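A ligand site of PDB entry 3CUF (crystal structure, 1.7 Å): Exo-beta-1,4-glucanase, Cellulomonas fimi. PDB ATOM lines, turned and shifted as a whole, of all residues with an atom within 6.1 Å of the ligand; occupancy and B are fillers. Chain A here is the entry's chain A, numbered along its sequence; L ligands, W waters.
The backbone NH (N) of Glu 233 sits close to the backbone carbonyl oxygen (O) of Gln 203 (2.9 Å). The side-chain carboxylate (OE2) of Glu 233 sits at hydrogen-bond distance from the side-chain amide nitrogen (ND2) of Asn 169 (3.0 Å). OE1 of Glu 127 is in hydrogen-bond range of NE1 of Trp 84, at 2.9 Å. The side-chain amino group (NZ) of Lys 47 is in hydrogen-bond range of the backbone carbonyl oxygen (O) of Glu 43 (3.0 Å). OD1 of Asn 126 sits at hydrogen-bond distance from NE2 of Gln 203 (3.1 Å). The side-chain carboxylate (OE2) of Glu 127 sits at hydrogen-bond distance from the side-chain amide nitrogen (NE2) of Gln 203, 2.9 Å away. The side-chain carboxylate (OE1) of Glu 233 lies within hydrogen-bond range of a ring nitrogen (NE2) of His 205 (2.8 Å). The indole nitrogen of Trp 84 lies close to the side-chain amide nitrogen of Asn 126, at 3.2 Å.
Water W3 bridges O4 of the ligand (2.6 Å) and OD1 of Asn 44 (2.9 Å). Water W2 bridges an oxygen (O2) of the ligand and the side-chain amide nitrogen (ND2) of Asn 44.
Trp 84 touches the ligand (CZ3 to O4, 3.5 Å). Gln 87 touches the ligand. ND2 of Asn 126 touches C9 of the ligand, 3.6 Å away. NE2 of His 205 touches C10 of the ligand, 3.7 Å away. Trp 281 touches the ligand. Hydrophobic or aromatic side chains that line the ligand: His 80, Trp 84, Trp 273 and Trp 281. 13 residues have an atom within 4 Å of the ligand: Glu 43, Asn 44, Lys 47, His 80, Trp 84, Gln 87, Asn 126, Glu 127, Gln 203, His 205, Glu 233, Trp 273 and Trp 281.
N1 of the ligand is in salt-bridge range of OE1 of Glu 233 (2.6 Å). ND2 of Asn 44 sits at hydrogen-bond distance from O2 of the ligand (3.0 Å). A nitrogen (N1) of the ligand is in hydrogen-bond range of the side-chain amide oxygen (OE1) of Gln 203, at 2.9 Å. NE1 of Trp 273 is in hydrogen-bond range of O1 of the ligand (2.8 Å). A nitrogen (N1) of the ligand is in salt-bridge range of the side-chain carboxylate of Glu 127 (2.9 Å). NE2 of His 80 sits at hydrogen-bond distance from O7 of the ligand, at 2.8 Å. OE2 of Glu 43 is in hydrogen-bond range of O1 of the ligand (2.8 Å). An oxygen (O5) of the ligand is in hydrogen-bond range of the side-chain amino group (NZ) of Lys 47 (2.7 Å).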
ATOM      1  N   GLU A  43       9.447 -12.808 -23.030  1.00  0.00           N
ATOM      2  CA  GLU A  43       9.895 -13.605 -21.911  1.00  0.00           C
ATOM      3  C   GLU A  43      11.183 -13.030 -21.311  1.00  0.00           C
ATOM      4  O   GLU A  43      11.328 -13.013 -20.078  1.00  0.00           O
ATOM      5  CB  GLU A  43      10.143 -15.061 -22.356  1.00  0.00           C
ATOM      6  CG  GLU A  43      10.439 -16.003 -21.172  1.00  0.00           C
ATOM      7  CD  GLU A  43      10.796 -17.420 -21.600  1.00  0.00           C
ATOM      8  OE1 GLU A  43      11.043 -17.627 -22.816  1.00  0.00           O
ATOM      9  OE2 GLU A  43      10.879 -18.290 -20.693  1.00  0.00           O
ATOM     10  N   ASN A  44      12.075 -12.545 -22.178  1.00  0.00           N
ATOM     11  CA  ASN A  44      13.421 -12.066 -21.787  1.00  0.00           C
ATOM     12  C   ASN A  44      13.887 -10.816 -22.529  1.00  0.00           C
ATOM     13  O   ASN A  44      14.727 -10.098 -22.016  1.00  0.00           O
ATOM     14  CB  ASN A  44      14.455 -13.177 -22.034  1.00  0.00           C
ATOM     15  CG  ASN A  44      14.361 -14.256 -21.005  1.00  0.00           C
ATOM     16  OD1 ASN A  44      14.484 -13.986 -19.809  1.00  0.00           O
ATOM     17  ND2 ASN A  44      14.122 -15.493 -21.443  1.00  0.00           N
ATOM     18  N   LYS A  47      14.077  -7.198 -20.810  1.00  0.00           N
ATOM     19  CA  LYS A  47      14.680  -7.061 -19.487  1.00  0.00           C
ATOM     20  C   LYS A  47      15.933  -6.184 -19.582  1.00  0.00           C
ATOM     21  O   LYS A  47      16.419  -5.879 -20.677  1.00  0.00           O
ATOM     22  CB  LYS A  47      15.029  -8.440 -18.918  1.00  0.00           C
ATOM     23  CG  LYS A  47      13.793  -9.245 -18.540  1.00  0.00           C
ATOM     24  CD  LYS A  47      14.126 -10.696 -18.276  1.00  0.00           C
ATOM     25  CE  LYS A  47      12.851 -11.425 -17.805  1.00  0.00           C
ATOM     26  NZ  LYS A  47      13.002 -12.925 -17.581  1.00  0.00           N
ATOM     27  N   ASP A  49      19.159  -6.681 -18.789  1.00  0.00           N
ATOM     28  CA  ASP A  49      20.328  -7.257 -19.473  1.00  0.00           C
ATOM     29  C   ASP A  49      20.189  -7.337 -20.994  1.00  0.00           C
ATOM     30  O   ASP A  49      21.183  -7.199 -21.744  1.00  0.00           O
ATOM     31  CB  ASP A  49      20.698  -8.630 -18.877  1.00  0.00           C
ATOM     32  CG  ASP A  49      19.627  -9.709 -19.077  1.00  0.00           C
ATOM     33  OD1 ASP A  49      18.457  -9.436 -19.437  1.00  0.00           O
ATOM     34  OD2 ASP A  49      19.980 -10.901 -18.832  1.00  0.00           O
ATOM     35  N   HIS A  80       7.627  -6.318 -20.132  1.00  0.00           N
ATOM     36  CA  HIS A  80       8.260  -6.939 -18.962  1.00  0.00           C
ATOM     37  C   HIS A  80       9.779  -6.853 -19.133  1.00  0.00           C
ATOM     38  O   HIS A  80      10.292  -7.387 -20.120  1.00  0.00           O
ATOM     39  CB  HIS A  80       7.798  -8.422 -18.950  1.00  0.00           C
ATOM     40  CG  HIS A  80       8.366  -9.233 -17.824  1.00  0.00           C
ATOM     41  ND1 HIS A  80       7.888  -9.160 -16.536  1.00  0.00           N
ATOM     42  CD2 HIS A  80       9.336 -10.167 -17.818  1.00  0.00           C
ATOM     43  CE1 HIS A  80       8.571 -10.000 -15.769  1.00  0.00           C
ATOM     44  NE2 HIS A  80       9.444 -10.642 -16.534  1.00  0.00           N
ATOM     45  N   THR A  81      10.553  -6.210 -18.222  1.00  0.00           N
ATOM     46  CA  THR A  81      10.115  -5.524 -17.009  1.00  0.00           C
ATOM     47  C   THR A  81      11.199  -4.478 -16.790  1.00  0.00           C
ATOM     48  O   THR A  81      12.361  -4.726 -17.085  1.00  0.00           O
ATOM     49  CB  THR A  81       9.963  -6.451 -15.748  1.00  0.00           C
ATOM     50  OG1 THR A  81       9.798  -5.625 -14.589  1.00  0.00           O
ATOM     51  CG2 THR A  81      11.172  -7.384 -15.542  1.00  0.00           C
ATOM     52  N   TRP A  84      13.965  -4.861 -12.018  1.00  0.00           N
ATOM     53  CA  TRP A  84      13.961  -6.220 -11.424  1.00  0.00           C
ATOM     54  C   TRP A  84      15.366  -6.527 -10.933  1.00  0.00           C
ATOM     55  O   TRP A  84      16.345  -6.250 -11.616  1.00  0.00           O
ATOM     56  CB  TRP A  84      13.597  -7.243 -12.495  1.00  0.00           C
ATOM     57  CG  TRP A  84      13.422  -8.652 -12.017  1.00  0.00           C
ATOM     58  CD1 TRP A  84      12.965  -9.062 -10.799  1.00  0.00           C
ATOM     59  CD2 TRP A  84      13.628  -9.848 -12.782  1.00  0.00           C
ATOM     60  NE1 TRP A  84      12.909 -10.440 -10.742  1.00  0.00           N
ATOM     61  CE2 TRP A  84      13.293 -10.938 -11.958  1.00  0.00           C
ATOM     62  CE3 TRP A  84      14.113 -10.093 -14.087  1.00  0.00           C
ATOM     63  CZ2 TRP A  84      13.422 -12.269 -12.385  1.00  0.00           C
ATOM     64  CZ3 TRP A  84      14.223 -11.421 -14.514  1.00  0.00           C
ATOM     65  CH2 TRP A  84      13.860 -12.494 -13.664  1.00  0.00           C
ATOM     66  N   SER A  86      16.857  -9.289 -10.540  1.00  0.00           N
ATOM     67  CA  SER A  86      17.489 -10.467 -11.121  1.00  0.00           C
ATOM     68  C   SER A  86      18.077 -10.141 -12.480  1.00  0.00           C
ATOM     69  O   SER A  86      17.531  -9.332 -13.234  1.00  0.00           O
ATOM     70  CB  SER A  86      16.495 -11.611 -11.231  1.00  0.00           C
ATOM     71  OG  SER A  86      17.190 -12.802 -11.581  1.00  0.00           O
ATOM     72  N   GLN A  87      19.205 -10.775 -12.767  1.00  0.00           N
ATOM     73  CA  GLN A  87      19.878 -10.631 -14.051  1.00  0.00           C
ATOM     74  C   GLN A  87      20.277  -9.191 -14.339  1.00  0.00           C
ATOM     75  O   GLN A  87      20.336  -8.783 -15.491  1.00  0.00           O
ATOM     76  CB  GLN A  87      18.982 -11.148 -15.195  1.00  0.00           C
ATOM     77  CG  GLN A  87      18.286 -12.490 -14.930  1.00  0.00           C
ATOM     78  CD  GLN A  87      19.274 -13.632 -14.835  1.00  0.00           C
ATOM     79  OE1 GLN A  87      20.008 -13.914 -15.780  1.00  0.00           O
ATOM     80  NE2 GLN A  87      19.297 -14.303 -13.676  1.00  0.00           N
ATOM     81  N   ASN A 126       9.222  -5.332 -10.667  1.00  0.00           N
ATOM     82  CA  ASN A 126       8.982  -6.762 -10.543  1.00  0.00           C
ATOM     83  C   ASN A 126       9.621  -7.341  -9.268  1.00  0.00           C
ATOM     84  O   ASN A 126      10.799  -7.063  -8.980  1.00  0.00           O
ATOM     85  CB  ASN A 126       9.557  -7.485 -11.779  1.00  0.00           C
ATOM     86  CG  ASN A 126       9.123  -8.943 -11.862  1.00  0.00           C
ATOM     87  OD1 ASN A 126       7.961  -9.278 -11.626  1.00  0.00           O
ATOM     88  ND2 ASN A 126      10.090  -9.830 -12.186  1.00  0.00           N
ATOM     89  N   GLU A 127       8.853  -8.155  -8.538  1.00  0.00           N
ATOM     90  CA  GLU A 127       9.373  -8.941  -7.373  1.00  0.00           C
ATOM     91  C   GLU A 127      10.057  -8.106  -6.283  1.00  0.00           C
ATOM     92  O   GLU A 127      11.161  -8.442  -5.803  1.00  0.00           O
ATOM     93  CB  GLU A 127      10.287 -10.068  -7.859  1.00  0.00           C
ATOM     94  CG  GLU A 127       9.539 -10.958  -8.849  1.00  0.00           C
ATOM     95  CD  GLU A 127      10.414 -12.050  -9.498  1.00  0.00           C
ATOM     96  OE1 GLU A 127      11.554 -12.312  -9.050  1.00  0.00           O
ATOM     97  OE2 GLU A 127       9.918 -12.638 -10.497  1.00  0.00           O
ATOM     98  N   ASN A 169       4.420  -6.195 -10.339  1.00  0.00           N
ATOM     99  CA  ASN A 169       4.206  -7.640 -10.567  1.00  0.00           C
ATOM    100  C   ASN A 169       4.948  -8.451  -9.488  1.00  0.00           C
ATOM    101  O   ASN A 169       6.021  -8.061  -9.033  1.00  0.00           O
ATOM    102  CB  ASN A 169       4.744  -7.946 -11.980  1.00  0.00           C
ATOM    103  CG  ASN A 169       4.433  -9.350 -12.463  1.00  0.00           C
ATOM    104  OD1 ASN A 169       3.269  -9.779 -12.464  1.00  0.00           O
ATOM    105  ND2 ASN A 169       5.486 -10.072 -12.894  1.00  0.00           N
ATOM    106  N   TYR A 171       5.255 -12.727  -7.407  1.00  0.00           N
ATOM    107  CA  TYR A 171       4.845 -14.136  -7.260  1.00  0.00           C
ATOM    108  C   TYR A 171       4.618 -14.476  -5.792  1.00  0.00           C
ATOM    109  O   TYR A 171       5.034 -13.737  -4.901  1.00  0.00           O
ATOM    110  CB  TYR A 171       5.893 -15.066  -7.898  1.00  0.00           C
ATOM    111  CG  TYR A 171       7.206 -15.081  -7.152  1.00  0.00           C
ATOM    112  CD1 TYR A 171       7.423 -15.972  -6.076  1.00  0.00           C
ATOM    113  CD2 TYR A 171       8.221 -14.209  -7.515  1.00  0.00           C
ATOM    114  CE1 TYR A 171       8.634 -15.994  -5.398  1.00  0.00           C
ATOM    115  CE2 TYR A 171       9.433 -14.221  -6.833  1.00  0.00           C
ATOM    116  CZ  TYR A 171       9.622 -15.099  -5.776  1.00  0.00           C
ATOM    117  OH  TYR A 171      10.835 -15.112  -5.094  1.00  0.00           O
ATOM    118  N   GLN A 203       1.915 -13.373 -10.766  1.00  0.00           N
ATOM    119  CA  GLN A 203       2.626 -14.242 -11.677  1.00  0.00           C
ATOM    120  C   GLN A 203       2.024 -15.628 -11.803  1.00  0.00           C
ATOM    121  O   GLN A 203       1.954 -16.187 -12.918  1.00  0.00           O
ATOM    122  CB  GLN A 203       4.079 -14.366 -11.245  1.00  0.00           C
ATOM    123  CG  GLN A 203       4.890 -13.104 -11.477  1.00  0.00           C
ATOM    124  CD  GLN A 203       6.354 -13.277 -11.064  1.00  0.00           C
ATOM    125  OE1 GLN A 203       6.866 -14.409 -10.995  1.00  0.00           O
ATOM    126  NE2 GLN A 203       7.035 -12.151 -10.833  1.00  0.00           N
ATOM    127  N   HIS A 205       3.089 -18.658 -10.751  1.00  0.00           N
ATOM    128  CA  HIS A 205       3.943 -19.842 -10.907  1.00  0.00           C
ATOM    129  C   HIS A 205       3.557 -20.843  -9.811  1.00  0.00           C
ATOM    130  O   HIS A 205       4.068 -20.789  -8.686  1.00  0.00           O
ATOM    131  CB  HIS A 205       5.430 -19.468 -10.839  1.00  0.00           C
ATOM    132  CG  HIS A 205       5.878 -18.629 -11.997  1.00  0.00           C
ATOM    133  ND1 HIS A 205       5.862 -19.095 -13.296  1.00  0.00           N
ATOM    134  CD2 HIS A 205       6.304 -17.338 -12.061  1.00  0.00           C
ATOM    135  CE1 HIS A 205       6.294 -18.138 -14.112  1.00  0.00           C
ATOM    136  NE2 HIS A 205       6.554 -17.067 -13.381  1.00  0.00           N
ATOM    137  N   GLU A 233       2.047 -14.688 -15.450  1.00  0.00           N
ATOM    138  CA  GLU A 233       3.076 -15.681 -15.812  1.00  0.00           C
ATOM    139  C   GLU A 233       2.640 -17.090 -15.449  1.00  0.00           C
ATOM    140  O   GLU A 233       3.439 -17.890 -14.948  1.00  0.00           O
ATOM    141  CB  GLU A 233       4.377 -15.339 -15.091  1.00  0.00           C
ATOM    142  CG  GLU A 233       4.811 -13.850 -15.180  1.00  0.00           C
ATOM    143  CD  GLU A 233       6.182 -13.541 -14.640  1.00  0.00           C
ATOM    144  OE1 GLU A 233       6.915 -14.495 -14.287  1.00  0.00           O
ATOM    145  OE2 GLU A 233       6.545 -12.342 -14.543  1.00  0.00           O
ATOM    146  N   TRP A 273       3.235 -18.507 -19.167  1.00  0.00           N
ATOM    147  CA  TRP A 273       4.663 -18.204 -19.266  1.00  0.00           C
ATOM    148  C   TRP A 273       5.366 -19.172 -20.252  1.00  0.00           C
ATOM    149  O   TRP A 273       6.299 -19.938 -19.907  1.00  0.00           O
ATOM    150  CB  TRP A 273       5.344 -18.182 -17.864  1.00  0.00           C
ATOM    151  CG  TRP A 273       6.599 -17.338 -17.885  1.00  0.00           C
ATOM    152  CD1 TRP A 273       7.886 -17.760 -17.663  1.00  0.00           C
ATOM    153  CD2 TRP A 273       6.674 -15.940 -18.172  1.00  0.00           C
ATOM    154  NE1 TRP A 273       8.753 -16.672 -17.776  1.00  0.00           N
ATOM    155  CE2 TRP A 273       8.029 -15.562 -18.084  1.00  0.00           C
ATOM    156  CE3 TRP A 273       5.723 -14.949 -18.467  1.00  0.00           C
ATOM    157  CZ2 TRP A 273       8.464 -14.250 -18.324  1.00  0.00           C
ATOM    158  CZ3 TRP A 273       6.167 -13.639 -18.707  1.00  0.00           C
ATOM    159  CH2 TRP A 273       7.531 -13.321 -18.611  1.00  0.00           C
ATOM    160  N   TRP A 281      11.004 -22.511 -18.663  1.00  0.00           N
ATOM    161  CA  TRP A 281      12.042 -22.230 -17.669  1.00  0.00           C
ATOM    162  C   TRP A 281      12.119 -23.253 -16.511  1.00  0.00           C
ATOM    163  O   TRP A 281      13.148 -23.374 -15.861  1.00  0.00           O
ATOM    164  CB  TRP A 281      11.818 -20.833 -17.050  1.00  0.00           C
ATOM    165  CG  TRP A 281      10.641 -20.791 -16.156  1.00  0.00           C
ATOM    166  CD1 TRP A 281       9.334 -20.801 -16.519  1.00  0.00           C
ATOM    167  CD2 TRP A 281      10.660 -20.765 -14.714  1.00  0.00           C
ATOM    168  NE1 TRP A 281       8.526 -20.773 -15.395  1.00  0.00           N
ATOM    169  CE2 TRP A 281       9.326 -20.754 -14.287  1.00  0.00           C
ATOM    170  CE3 TRP A 281      11.694 -20.768 -13.754  1.00  0.00           C
ATOM    171  CZ2 TRP A 281       8.968 -20.736 -12.922  1.00  0.00           C
ATOM    172  CZ3 TRP A 281      11.347 -20.749 -12.398  1.00  0.00           C
ATOM    173  CH2 TRP A 281       9.984 -20.733 -11.993  1.00  0.00           C
ATOM    174  N   VAL A 285      15.429 -24.729 -13.383  1.00  0.00           N
ATOM    175  CA  VAL A 285      15.415 -24.150 -12.051  1.00  0.00           C
ATOM    176  C   VAL A 285      15.071 -25.201 -10.982  1.00  0.00           C
ATOM    177  O   VAL A 285      15.656 -25.193  -9.912  1.00  0.00           O
ATOM    178  CB  VAL A 285      14.459 -22.923 -11.975  1.00  0.00           C
ATOM    179  CG1 VAL A 285      14.246 -22.463 -10.517  1.00  0.00           C
ATOM    180  CG2 VAL A 285      15.007 -21.789 -12.812  1.00  0.00           C
HETATM  181  O1  LIG L   1      11.353 -17.544 -18.059  1.00  0.00           O
HETATM  182  C1  LIG L   1      12.514 -16.684 -17.876  1.00  0.00           C
HETATM  183  C2  LIG L   1      13.845 -17.412 -18.083  1.00  0.00           C
HETATM  184  O2  LIG L   1      13.972 -17.733 -19.470  1.00  0.00           O
HETATM  185  C3  LIG L   1      15.026 -16.525 -17.669  1.00  0.00           C
HETATM  186  O3  LIG L   1      16.235 -17.326 -17.636  1.00  0.00           O
HETATM  187  C4  LIG L   1      14.803 -15.859 -16.300  1.00  0.00           C
HETATM  188  C5  LIG L   1      15.817 -14.742 -15.960  1.00  0.00           C
HETATM  189  O4  LIG L   1      15.667 -13.639 -16.842  1.00  0.00           O
HETATM  190  O5  LIG L   1      13.515 -15.200 -16.303  1.00  0.00           O
HETATM  191  C6  LIG L   1      12.497 -16.159 -16.447  1.00  0.00           C
HETATM  192  O6  LIG L   1      11.244 -15.461 -16.353  1.00  0.00           O
HETATM  193  C7  LIG L   1      10.931 -15.055 -14.984  1.00  0.00           C
HETATM  194  C8  LIG L   1      10.152 -13.728 -15.108  1.00  0.00           C
HETATM  195  O7  LIG L   1      11.004 -12.790 -15.777  1.00  0.00           O
HETATM  196  C9  LIG L   1       9.817 -13.121 -13.733  1.00  0.00           C
HETATM  197  N1  LIG L   1       9.105 -14.098 -12.880  1.00  0.00           N
HETATM  198  C10 LIG L   1       9.794 -15.417 -12.762  1.00  0.00           C
HETATM  199  C11 LIG L   1      10.048 -16.023 -14.156  1.00  0.00           C
HETATM  200  C12 LIG L   1      10.610 -17.462 -13.993  1.00  0.00           C
HETATM  201  O8  LIG L   1      11.871 -17.438 -13.313  1.00  0.00           O
HETATM  202  O   HOH W   1      14.626 -20.368 -19.670  1.00  0.00           O
HETATM  203  O   HOH W   2      16.629 -17.784 -21.309  1.00  0.00           O
HETATM  204  O   HOH W   3      17.241 -13.473 -18.925  1.00  0.00           O
HETATM  205  O   HOH W   4       8.871 -16.094  -9.766  1.00  0.00           O
HETATM  206  O   HOH W   5      15.611 -19.438 -15.704  1.00  0.00           O
HETATM  207  O   HOH W   6      14.306 -18.512 -13.873  1.00  0.00           O
